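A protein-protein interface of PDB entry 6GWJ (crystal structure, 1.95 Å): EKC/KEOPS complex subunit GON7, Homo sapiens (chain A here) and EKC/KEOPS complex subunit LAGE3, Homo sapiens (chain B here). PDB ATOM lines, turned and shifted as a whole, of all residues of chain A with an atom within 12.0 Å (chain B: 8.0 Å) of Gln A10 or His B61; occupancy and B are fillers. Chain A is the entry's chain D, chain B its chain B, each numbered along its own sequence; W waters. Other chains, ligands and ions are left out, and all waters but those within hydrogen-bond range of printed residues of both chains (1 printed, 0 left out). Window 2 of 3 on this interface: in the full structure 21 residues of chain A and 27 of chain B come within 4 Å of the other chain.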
ATOM      1  N   GLY A   5      16.292  28.399 -16.104  1.00  0.00           N
ATOM      2  CA  GLY A   5      16.921  28.211 -17.399  1.00  0.00           C
ATOM      3  C   GLY A   5      15.889  28.215 -18.504  1.00  0.00           C
ATOM      4  O   GLY A   5      14.790  27.687 -18.323  1.00  0.00           O
ATOM      5  N   GLU A   6      16.224  28.822 -19.646  1.00  0.00           N
ATOM      6  CA  GLU A   6      15.320  28.856 -20.785  1.00  0.00           C
ATOM      7  C   GLU A   6      16.039  28.402 -22.043  1.00  0.00           C
ATOM      8  O   GLU A   6      16.993  29.059 -22.482  1.00  0.00           O
ATOM      9  CB  GLU A   6      14.684  30.246 -20.980  1.00  0.00           C
ATOM     10  CG  GLU A   6      13.506  30.212 -21.950  1.00  0.00           C
ATOM     11  CD  GLU A   6      12.941  31.541 -22.417  1.00  0.00           C
ATOM     12  OE1 GLU A   6      12.589  32.384 -21.557  1.00  0.00           O
ATOM     13  OE2 GLU A   6      12.778  31.708 -23.647  1.00  0.00           O
ATOM     14  N   TYR A   7      15.593  27.268 -22.614  1.00  0.00           N
ATOM     15  CA  TYR A   7      16.160  26.757 -23.855  1.00  0.00           C
ATOM     16  C   TYR A   7      15.247  27.100 -25.029  1.00  0.00           C
ATOM     17  O   TYR A   7      14.039  26.858 -24.964  1.00  0.00           O
ATOM     18  CB  TYR A   7      16.435  25.244 -23.787  1.00  0.00           C
ATOM     19  CG  TYR A   7      16.839  24.631 -25.114  1.00  0.00           C
ATOM     20  CD1 TYR A   7      18.111  24.842 -25.643  1.00  0.00           C
ATOM     21  CD2 TYR A   7      15.944  23.862 -25.854  1.00  0.00           C
ATOM     22  CE1 TYR A   7      18.482  24.299 -26.875  1.00  0.00           C
ATOM     23  CE2 TYR A   7      16.304  23.314 -27.085  1.00  0.00           C
ATOM     24  CZ  TYR A   7      17.576  23.531 -27.589  1.00  0.00           C
ATOM     25  OH  TYR A   7      17.939  22.980 -28.795  1.00  0.00           O
ATOM     26  N   VAL A   8      15.831  27.672 -26.096  1.00  0.00           N
ATOM     27  CA  VAL A   8      15.118  28.003 -27.330  1.00  0.00           C
ATOM     28  C   VAL A   8      15.934  27.391 -28.481  1.00  0.00           C
ATOM     29  O   VAL A   8      17.040  27.852 -28.790  1.00  0.00           O
ATOM     30  CB  VAL A   8      14.826  29.519 -27.540  1.00  0.00           C
ATOM     31  CG1 VAL A   8      13.871  29.735 -28.715  1.00  0.00           C
ATOM     32  CG2 VAL A   8      14.264  30.169 -26.276  1.00  0.00           C
ATOM     33  N   GLY A   9      15.396  26.325 -29.063  1.00  0.00           N
ATOM     34  CA  GLY A   9      16.034  25.625 -30.170  1.00  0.00           C
ATOM     35  C   GLY A   9      15.937  26.383 -31.479  1.00  0.00           C
ATOM     36  O   GLY A   9      15.305  27.444 -31.549  1.00  0.00           O
ATOM     37  N   GLN A  10      16.549  25.821 -32.537  1.00  0.00           N
ATOM     38  CA  GLN A  10      16.541  26.393 -33.889  1.00  0.00           C
ATOM     39  C   GLN A  10      15.126  26.443 -34.481  1.00  0.00           C
ATOM     40  O   GLN A  10      14.853  27.283 -35.341  1.00  0.00           O
ATOM     41  CB  GLN A  10      17.519  25.645 -34.810  1.00  0.00           C
ATOM     42  CG  GLN A  10      18.986  25.864 -34.424  1.00  0.00           C
ATOM     43  CD  GLN A  10      19.966  25.066 -35.252  1.00  0.00           C
ATOM     44  OE1 GLN A  10      19.739  23.897 -35.599  1.00  0.00           O
ATOM     45  NE2 GLN A  10      21.117  25.665 -35.520  1.00  0.00           N
ATOM     46  N   GLU A  11      14.224  25.572 -33.979  1.00  0.00           N
ATOM     47  CA  GLU A  11      12.813  25.492 -34.369  1.00  0.00           C
ATOM     48  C   GLU A  11      11.976  26.657 -33.794  1.00  0.00           C
ATOM     49  O   GLU A  11      10.959  27.023 -34.390  1.00  0.00           O
ATOM     50  CB  GLU A  11      12.209  24.110 -34.007  1.00  0.00           C
ATOM     51  CG  GLU A  11      11.905  23.857 -32.528  1.00  0.00           C
ATOM     52  CD  GLU A  11      13.067  23.784 -31.553  1.00  0.00           C
ATOM     53  OE1 GLU A  11      14.128  23.226 -31.915  1.00  0.00           O
ATOM     54  OE2 GLU A  11      12.899  24.254 -30.406  1.00  0.00           O
ATOM     55  N   GLY A  12      12.413  27.207 -32.655  1.00  0.00           N
ATOM     56  CA  GLY A  12      11.757  28.320 -31.972  1.00  0.00           C
ATOM     57  C   GLY A  12      10.886  27.948 -30.785  1.00  0.00           C
ATOM     58  O   GLY A  12      10.345  28.841 -30.123  1.00  0.00           O
ATOM     59  N   LYS A  13      10.736  26.632 -30.502  1.00  0.00           N
ATOM     60  CA  LYS A  13       9.930  26.114 -29.385  1.00  0.00           C
ATOM     61  C   LYS A  13      10.662  26.327 -28.036  1.00  0.00           C
ATOM     62  O   LYS A  13      11.736  25.748 -27.835  1.00  0.00           O
ATOM     63  CB  LYS A  13       9.583  24.627 -29.596  1.00  0.00           C
ATOM     64  CG  LYS A  13       8.577  24.362 -30.717  1.00  0.00           C
ATOM     65  CD  LYS A  13       8.507  22.880 -31.103  1.00  0.00           C
ATOM     66  CE  LYS A  13       7.520  22.087 -30.276  1.00  0.00           C
ATOM     67  NZ  LYS A  13       7.529  20.647 -30.644  1.00  0.00           N
ATOM     68  N   PRO A  14      10.117  27.159 -27.108  1.00  0.00           N
ATOM     69  CA  PRO A  14      10.825  27.401 -25.839  1.00  0.00           C
ATOM     70  C   PRO A  14      10.507  26.415 -24.714  1.00  0.00           C
ATOM     71  O   PRO A  14       9.337  26.141 -24.432  1.00  0.00           O
ATOM     72  CB  PRO A  14      10.427  28.836 -25.480  1.00  0.00           C
ATOM     73  CG  PRO A  14       9.118  29.079 -26.201  1.00  0.00           C
ATOM     74  CD  PRO A  14       8.874  27.954 -27.181  1.00  0.00           C
ATOM     75  N   GLN A  15      11.564  25.892 -24.063  1.00  0.00           N
ATOM     76  CA  GLN A  15      11.463  24.954 -22.943  1.00  0.00           C
ATOM     77  C   GLN A  15      12.064  25.585 -21.684  1.00  0.00           C
ATOM     78  O   GLN A  15      13.225  26.010 -21.696  1.00  0.00           O
ATOM     79  CB  GLN A  15      12.150  23.613 -23.270  1.00  0.00           C
ATOM     80  CG  GLN A  15      11.430  22.786 -24.333  1.00  0.00           C
ATOM     81  CD  GLN A  15      12.108  21.458 -24.547  1.00  0.00           C
ATOM     82  OE1 GLN A  15      11.873  20.489 -23.816  1.00  0.00           O
ATOM     83  NE2 GLN A  15      12.967  21.384 -25.554  1.00  0.00           N
ATOM     84  N   VAL A  44      19.232  20.294 -16.694  1.00  0.00           N
ATOM     85  CA  VAL A  44      19.939  20.576 -17.947  1.00  0.00           C
ATOM     86  C   VAL A  44      20.318  19.231 -18.605  1.00  0.00           C
ATOM     87  O   VAL A  44      20.092  19.060 -19.801  1.00  0.00           O
ATOM     88  CB  VAL A  44      21.160  21.537 -17.741  1.00  0.00           C
ATOM     89  CG1 VAL A  44      22.044  21.607 -18.992  1.00  0.00           C
ATOM     90  CG2 VAL A  44      20.689  22.940 -17.353  1.00  0.00           C
ATOM     91  N   LEU A  47      17.123  17.644 -19.975  1.00  0.00           N
ATOM     92  CA  LEU A  47      16.601  18.399 -21.116  1.00  0.00           C
ATOM     93  C   LEU A  47      17.358  18.070 -22.413  1.00  0.00           C
ATOM     94  O   LEU A  47      16.722  17.794 -23.430  1.00  0.00           O
ATOM     95  CB  LEU A  47      16.664  19.909 -20.815  1.00  0.00           C
ATOM     96  CG  LEU A  47      16.137  20.883 -21.866  1.00  0.00           C
ATOM     97  CD1 LEU A  47      14.614  20.931 -21.856  1.00  0.00           C
ATOM     98  CD2 LEU A  47      16.685  22.276 -21.614  1.00  0.00           C
ATOM     99  N   PHE A  48      18.705  18.067 -22.360  1.00  0.00           N
ATOM    100  CA  PHE A  48      19.563  17.837 -23.520  1.00  0.00           C
ATOM    101  C   PHE A  48      19.830  16.360 -23.883  1.00  0.00           C
ATOM    102  O   PHE A  48      20.160  16.102 -25.042  1.00  0.00           O
ATOM    103  CB  PHE A  48      20.887  18.597 -23.364  1.00  0.00           C
ATOM    104  CG  PHE A  48      20.750  20.100 -23.471  1.00  0.00           C
ATOM    105  CD1 PHE A  48      20.669  20.724 -24.711  1.00  0.00           C
ATOM    106  CD2 PHE A  48      20.714  20.894 -22.332  1.00  0.00           C
ATOM    107  CE1 PHE A  48      20.543  22.114 -24.806  1.00  0.00           C
ATOM    108  CE2 PHE A  48      20.590  22.285 -22.429  1.00  0.00           C
ATOM    109  CZ  PHE A  48      20.509  22.884 -23.663  1.00  0.00           C
ATOM    110  N   ASP A  49      19.695  15.401 -22.937  1.00  0.00           N
ATOM    111  CA  ASP A  49      19.939  13.975 -23.235  1.00  0.00           C
ATOM    112  C   ASP A  49      18.997  13.407 -24.345  1.00  0.00           C
ATOM    113  O   ASP A  49      19.538  12.887 -25.325  1.00  0.00           O
ATOM    114  CB  ASP A  49      19.938  13.090 -21.970  1.00  0.00           C
ATOM    115  CG  ASP A  49      21.243  13.099 -21.171  1.00  0.00           C
ATOM    116  OD1 ASP A  49      22.096  13.994 -21.416  1.00  0.00           O
ATOM    117  OD2 ASP A  49      21.395  12.237 -20.275  1.00  0.00           O
ATOM    118  N   PRO A  50      17.639  13.537 -24.295  1.00  0.00           N
ATOM    119  CA  PRO A  50      16.831  13.020 -25.416  1.00  0.00           C
ATOM    120  C   PRO A  50      16.753  13.997 -26.592  1.00  0.00           C
ATOM    121  O   PRO A  50      16.679  15.214 -26.406  1.00  0.00           O
ATOM    122  CB  PRO A  50      15.461  12.761 -24.783  1.00  0.00           C
ATOM    123  CG  PRO A  50      15.383  13.708 -23.629  1.00  0.00           C
ATOM    124  CD  PRO A  50      16.779  14.131 -23.248  1.00  0.00           C
ATOM    125  N   PRO B  60      19.787  29.900 -34.230  1.00  0.00           N
ATOM    126  CA  PRO B  60      20.747  29.197 -33.360  1.00  0.00           C
ATOM    127  C   PRO B  60      20.147  28.719 -32.039  1.00  0.00           C
ATOM    128  O   PRO B  60      19.122  29.254 -31.594  1.00  0.00           O
ATOM    129  CB  PRO B  60      21.851  30.240 -33.123  1.00  0.00           C
ATOM    130  CG  PRO B  60      21.192  31.557 -33.358  1.00  0.00           C
ATOM    131  CD  PRO B  60      20.165  31.311 -34.439  1.00  0.00           C
ATOM    132  N   HIS B  61      20.811  27.720 -31.402  1.00  0.00           N
ATOM    133  CA  HIS B  61      20.415  27.165 -30.106  1.00  0.00           C
ATOM    134  C   HIS B  61      20.755  28.204 -29.036  1.00  0.00           C
ATOM    135  O   HIS B  61      21.883  28.713 -28.996  1.00  0.00           O
ATOM    136  CB  HIS B  61      21.138  25.836 -29.819  1.00  0.00           C
ATOM    137  CG  HIS B  61      20.875  24.764 -30.828  1.00  0.00           C
ATOM    138  ND1 HIS B  61      21.809  24.441 -31.803  1.00  0.00           N
ATOM    139  CD2 HIS B  61      19.793  23.967 -30.982  1.00  0.00           C
ATOM    140  CE1 HIS B  61      21.268  23.459 -32.506  1.00  0.00           C
ATOM    141  NE2 HIS B  61      20.056  23.139 -32.049  1.00  0.00           N
ATOM    142  N   ILE B  62      19.755  28.565 -28.214  1.00  0.00           N
ATOM    143  CA  ILE B  62      19.902  29.591 -27.184  1.00  0.00           C
ATOM    144  C   ILE B  62      19.568  29.044 -25.797  1.00  0.00           C
ATOM    145  O   ILE B  62      18.578  28.335 -25.633  1.00  0.00           O
ATOM    146  CB  ILE B  62      19.070  30.858 -27.583  1.00  0.00           C
ATOM    147  CG1 ILE B  62      19.796  31.656 -28.706  1.00  0.00           C
ATOM    148  CG2 ILE B  62      18.748  31.770 -26.374  1.00  0.00           C
ATOM    149  CD1 ILE B  62      18.919  32.529 -29.583  1.00  0.00           C
ATOM    150  N   PHE B  63      20.402  29.379 -24.803  1.00  0.00           N
ATOM    151  CA  PHE B  63      20.160  29.023 -23.406  1.00  0.00           C
ATOM    152  C   PHE B  63      20.416  30.225 -22.514  1.00  0.00           C
ATOM    153  O   PHE B  63      21.486  30.826 -22.592  1.00  0.00           O
ATOM    154  CB  PHE B  63      20.970  27.791 -22.939  1.00  0.00           C
ATOM    155  CG  PHE B  63      20.454  27.216 -21.633  1.00  0.00           C
ATOM    156  CD1 PHE B  63      19.409  26.295 -21.623  1.00  0.00           C
ATOM    157  CD2 PHE B  63      20.987  27.623 -20.414  1.00  0.00           C
ATOM    158  CE1 PHE B  63      18.915  25.780 -20.416  1.00  0.00           C
ATOM    159  CE2 PHE B  63      20.494  27.110 -19.208  1.00  0.00           C
ATOM    160  CZ  PHE B  63      19.458  26.192 -19.218  1.00  0.00           C
ATOM    161  N   THR B  64      19.441  30.572 -21.662  1.00  0.00           N
ATOM    162  CA  THR B  64      19.566  31.694 -20.727  1.00  0.00           C
ATOM    163  C   THR B  64      19.392  31.194 -19.304  1.00  0.00           C
ATOM    164  O   THR B  64      18.400  30.538 -19.013  1.00  0.00           O
ATOM    165  CB  THR B  64      18.569  32.823 -21.071  1.00  0.00           C
ATOM    166  OG1 THR B  64      18.707  33.178 -22.449  1.00  0.00           O
ATOM    167  CG2 THR B  64      18.752  34.061 -20.184  1.00  0.00           C
ATOM    168  N   VAL B  92      31.726  27.772 -32.087  1.00  0.00           N
ATOM    169  CA  VAL B  92      30.618  26.825 -31.889  1.00  0.00           C
ATOM    170  C   VAL B  92      29.656  27.248 -30.758  1.00  0.00           C
ATOM    171  O   VAL B  92      28.438  27.163 -30.926  1.00  0.00           O
ATOM    172  CB  VAL B  92      31.178  25.383 -31.682  1.00  0.00           C
ATOM    173  CG1 VAL B  92      30.070  24.383 -31.355  1.00  0.00           C
ATOM    174  CG2 VAL B  92      31.968  24.927 -32.910  1.00  0.00           C
ATOM    175  N   VAL B  93      30.212  27.637 -29.599  1.00  0.00           N
ATOM    176  CA  VAL B  93      29.460  28.039 -28.409  1.00  0.00           C
ATOM    177  C   VAL B  93      30.056  29.338 -27.854  1.00  0.00           C
ATOM    178  O   VAL B  93      31.261  29.412 -27.586  1.00  0.00           O
ATOM    179  CB  VAL B  93      29.418  26.924 -27.306  1.00  0.00           C
ATOM    180  CG1 VAL B  93      28.640  27.384 -26.071  1.00  0.00           C
ATOM    181  CG2 VAL B  93      28.844  25.612 -27.838  1.00  0.00           C
ATOM    182  N   GLY B  94      29.191  30.322 -27.658  1.00  0.00           N
ATOM    183  CA  GLY B  94      29.543  31.598 -27.059  1.00  0.00           C
ATOM    184  C   GLY B  94      28.606  31.929 -25.914  1.00  0.00           C
ATOM    185  O   GLY B  94      27.451  31.487 -25.911  1.00  0.00           O
ATOM    186  N   ARG B 107      23.849  34.284 -20.862  1.00  0.00           N
ATOM    187  CA  ARG B 107      23.214  34.077 -22.150  1.00  0.00           C
ATOM    188  C   ARG B 107      24.141  33.320 -23.092  1.00  0.00           C
ATOM    189  O   ARG B 107      25.225  33.811 -23.413  1.00  0.00           O
ATOM    190  CB  ARG B 107      22.766  35.426 -22.738  1.00  0.00           C
ATOM    191  CG  ARG B 107      21.618  36.066 -21.947  1.00  0.00           C
ATOM    192  CD  ARG B 107      20.987  37.249 -22.665  1.00  0.00           C
ATOM    193  NE  ARG B 107      19.800  37.739 -21.958  1.00  0.00           N
ATOM    194  CZ  ARG B 107      19.813  38.698 -21.036  1.00  0.00           C
ATOM    195  NH1 ARG B 107      18.686  39.071 -20.443  1.00  0.00           N
ATOM    196  NH2 ARG B 107      20.953  39.282 -20.688  1.00  0.00           N
ATOM    197  N   TRP B 108      23.721  32.113 -23.506  1.00  0.00           N
ATOM    198  CA  TRP B 108      24.463  31.252 -24.435  1.00  0.00           C
ATOM    199  C   TRP B 108      23.860  31.292 -25.852  1.00  0.00           C
ATOM    200  O   TRP B 108      22.642  31.358 -26.019  1.00  0.00           O
ATOM    201  CB  TRP B 108      24.456  29.791 -23.966  1.00  0.00           C
ATOM    202  CG  TRP B 108      25.422  29.423 -22.879  1.00  0.00           C
ATOM    203  CD1 TRP B 108      26.686  28.930 -23.035  1.00  0.00           C
ATOM    204  CD2 TRP B 108      25.156  29.407 -21.471  1.00  0.00           C
ATOM    205  NE1 TRP B 108      27.238  28.644 -21.804  1.00  0.00           N
ATOM    206  CE2 TRP B 108      26.316  28.917 -20.828  1.00  0.00           C
ATOM    207  CE3 TRP B 108      24.046  29.768 -20.683  1.00  0.00           C
ATOM    208  CZ2 TRP B 108      26.402  28.783 -19.437  1.00  0.00           C
ATOM    209  CZ3 TRP B 108      24.122  29.595 -19.306  1.00  0.00           C
ATOM    210  CH2 TRP B 108      25.294  29.118 -18.696  1.00  0.00           C
ATOM    211  N   LYS B 109      24.735  31.210 -26.863  1.00  0.00           N
ATOM    212  CA  LYS B 109      24.397  31.118 -28.285  1.00  0.00           C
ATOM    213  C   LYS B 109      25.262  29.976 -28.817  1.00  0.00           C
ATOM    214  O   LYS B 109      26.490  29.993 -28.625  1.00  0.00           O
ATOM    215  CB  LYS B 109      24.687  32.432 -29.032  1.00  0.00           C
ATOM    216  CG  LYS B 109      23.555  33.446 -28.951  1.00  0.00           C
ATOM    217  CD  LYS B 109      23.989  34.799 -29.520  1.00  0.00           C
ATOM    218  CE  LYS B 109      22.940  35.874 -29.359  1.00  0.00           C
ATOM    219  NZ  LYS B 109      21.832  35.729 -30.342  1.00  0.00           N
ATOM    220  N   ALA B 110      24.623  28.947 -29.397  1.00  0.00           N
ATOM    221  CA  ALA B 110      25.331  27.762 -29.876  1.00  0.00           C
ATOM    222  C   ALA B 110      24.860  27.203 -31.220  1.00  0.00           C
ATOM    223  O   ALA B 110      23.677  27.277 -31.569  1.00  0.00           O
ATOM    224  CB  ALA B 110      25.285  26.670 -28.816  1.00  0.00           C
ATOM    225  N   GLU B 111      25.817  26.616 -31.965  1.00  0.00           N
ATOM    226  CA  GLU B 111      25.602  25.949 -33.254  1.00  0.00           C
ATOM    227  C   GLU B 111      25.357  24.443 -33.017  1.00  0.00           C
ATOM    228  O   GLU B 111      24.710  23.793 -33.840  1.00  0.00           O
ATOM    229  CB  GLU B 111      26.830  26.132 -34.170  1.00  0.00           C
ATOM    230  CG  GLU B 111      27.149  27.571 -34.545  1.00  0.00           C
ATOM    231  CD  GLU B 111      26.380  28.108 -35.732  1.00  0.00           C
ATOM    232  OE1 GLU B 111      26.975  28.194 -36.831  1.00  0.00           O
ATOM    233  OE2 GLU B 111      25.182  28.432 -35.571  1.00  0.00           O
ATOM    234  N   ASP B 112      25.888  23.897 -31.892  1.00  0.00           N
ATOM    235  CA  ASP B 112      25.775  22.480 -31.534  1.00  0.00           C
ATOM    236  C   ASP B 112      25.090  22.298 -30.179  1.00  0.00           C
ATOM    237  O   ASP B 112      25.424  22.996 -29.222  1.00  0.00           O
ATOM    238  CB  ASP B 112      27.166  21.825 -31.525  1.00  0.00           C
ATOM    239  CG  ASP B 112      27.141  20.334 -31.238  1.00  0.00           C
ATOM    240  OD1 ASP B 112      26.593  19.587 -32.061  1.00  0.00           O
ATOM    241  OD2 ASP B 112      27.685  19.921 -30.195  1.00  0.00           O
ATOM    242  N   CYS B 113      24.154  21.340 -30.105  1.00  0.00           N
ATOM    243  CA  CYS B 113      23.371  21.034 -28.907  1.00  0.00           C
ATOM    244  C   CYS B 113      24.169  20.354 -27.802  1.00  0.00           C
ATOM    245  O   CYS B 113      23.985  20.704 -26.638  1.00  0.00           O
ATOM    246  CB  CYS B 113      22.128  20.230 -29.266  1.00  0.00           C
ATOM    247  SG  CYS B 113      20.577  21.050 -28.826  1.00  0.00           S
ATOM    248  N   ARG B 114      24.998  19.347 -28.150  1.00  0.00           N
ATOM    249  CA  ARG B 114      25.824  18.617 -27.185  1.00  0.00           C
ATOM    250  C   ARG B 114      26.851  19.561 -26.539  1.00  0.00           C
ATOM    251  O   ARG B 114      27.006  19.549 -25.312  1.00  0.00           O
ATOM    252  CB  ARG B 114      26.528  17.427 -27.853  1.00  0.00           C
ATOM    253  CG  ARG B 114      27.287  16.548 -26.869  1.00  0.00           C
ATOM    254  CD  ARG B 114      28.209  15.582 -27.576  1.00  0.00           C
ATOM    255  NE  ARG B 114      29.547  15.616 -26.988  1.00  0.00           N
ATOM    256  CZ  ARG B 114      30.586  16.247 -27.524  1.00  0.00           C
ATOM    257  NH1 ARG B 114      31.765  16.226 -26.919  1.00  0.00           N
ATOM    258  NH2 ARG B 114      30.461  16.885 -28.681  1.00  0.00           N
ATOM    259  N   LEU B 116      26.600  22.776 -26.288  1.00  0.00           N
ATOM    260  CA  LEU B 116      25.855  23.752 -25.480  1.00  0.00           C
ATOM    261  C   LEU B 116      25.581  23.145 -24.082  1.00  0.00           C
ATOM    262  O   LEU B 116      25.799  23.821 -23.078  1.00  0.00           O
ATOM    263  CB  LEU B 116      24.540  24.163 -26.170  1.00  0.00           C
ATOM    264  CG  LEU B 116      23.508  24.940 -25.331  1.00  0.00           C
ATOM    265  CD1 LEU B 116      24.086  26.250 -24.780  1.00  0.00           C
ATOM    266  CD2 LEU B 116      22.244  25.192 -26.127  1.00  0.00           C
HETATM  267  O   HOH W   1      23.285  24.017 -36.145  1.00  0.00           O
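The backbone carbonyl oxygen (O) of His B61 lies within hydrogen-bond range of the backbone NH (N) of Ala B110, at 2.8 Å.
N of Trp B108 sits at hydrogen-bond distance from O of Phe B63, at 2.7 Å.
The backbone carbonyl oxygen of Tyr A7 sits at hydrogen-bond distance from the backbone NH of Gln A15 (2.8 Å).
Water W1 lies within hydrogen-bond range of the backbone carbonyl oxygen (O) of Glu B111 (2.7 Å) and the side-chain amide nitrogen (NE2) of Gln A10 (2.8 Å).
Among the printed residues, merely in contact across the chains: Tyr A7 with His B61 (3.0 Å), Gly A5 with Thr B64 (3.2 Å), Glu A6 with Phe B63 (3.3 Å), Tyr A7 with Ile B62 (3.4 Å), Gln A10 with His B61 (3.4 Å), Glu A6 with Ile B62 (3.6 Å), Val A8 with His B61 (3.7 Å), Gly A5 with Phe B63 (3.7 Å), Phe A48 with Leu B116 (3.8 Å), Val A8 with Pro B60 (3.8 Å), Tyr A7 with Phe B63 (3.8 Å), Phe A48 with Cys B113 (3.8 Å), Gln A10 with Pro B60 (3.9 Å), Tyr A7 with Leu B116 (3.9 Å) and Val A44 with Phe B63 (3.9 Å).
N of Val A8 lies within hydrogen-bond range of O of Ile B62 (2.9 Å).
The backbone NH of Glu A6 is in hydrogen-bond range of the backbone carbonyl oxygen of Thr B64, 2.8 Å away.
OH of Tyr A7 lies within hydrogen-bond range of SG of Cys B113 (3.3 Å).
Printed residues of chain B that touch a printed residue of chain A: Pro B60, His B61, Ile B62, Phe B63, Thr B64, Cys B113 and Leu B116.
Hydrophobic or aromatic side chains of chain B within 4 Å of the printed part of chain A: His B61, Ile B62, Phe B63 and Leu B116.
Of the 16 printed residues of chain A, 7 touch a printed residue of chain B.
Gln A10 touches two residues of chain B.
His B61 touches three residues of chain A.
No residue of chain B comes within 4 Å of Gly A9.
Pro B60 touches two residues of chain A.
Ile B62 touches three residues of chain A.
No residue of chain A comes within 4 Å of Lys B109.
No residue of chain A comes within 4 Å of Ala B110.
No residue of chain A comes within 4 Å of Glu B111.
No residue of chain A comes within 4 Å of Asp B112.
Of the printed residues of chain A, Cys B113 touches Tyr A7 (3.3 Å) and Phe A48 (3.8 Å).
Printed residues of chain A within 4 Å of Thr B64: Gly A5 and Glu A6.
Printed residues of chain B within 4 Å of Glu A6: Ile B62 (3.6 Å), Phe B63 (3.3 Å) and Thr B64 (2.8 Å).
Of the printed residues of chain B, Val A8 touches Pro B60 (3.8 Å), His B61 (3.7 Å) and Ile B62 (2.9 Å).
Printed residues of chain B within 4 Å of Val A44: Phe B63.
Arg B107 touches none of the printed residues of chain A.
The nearest printed residue of chain B that does not touch Phe A48 is Phe B63 (4.1 Å).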
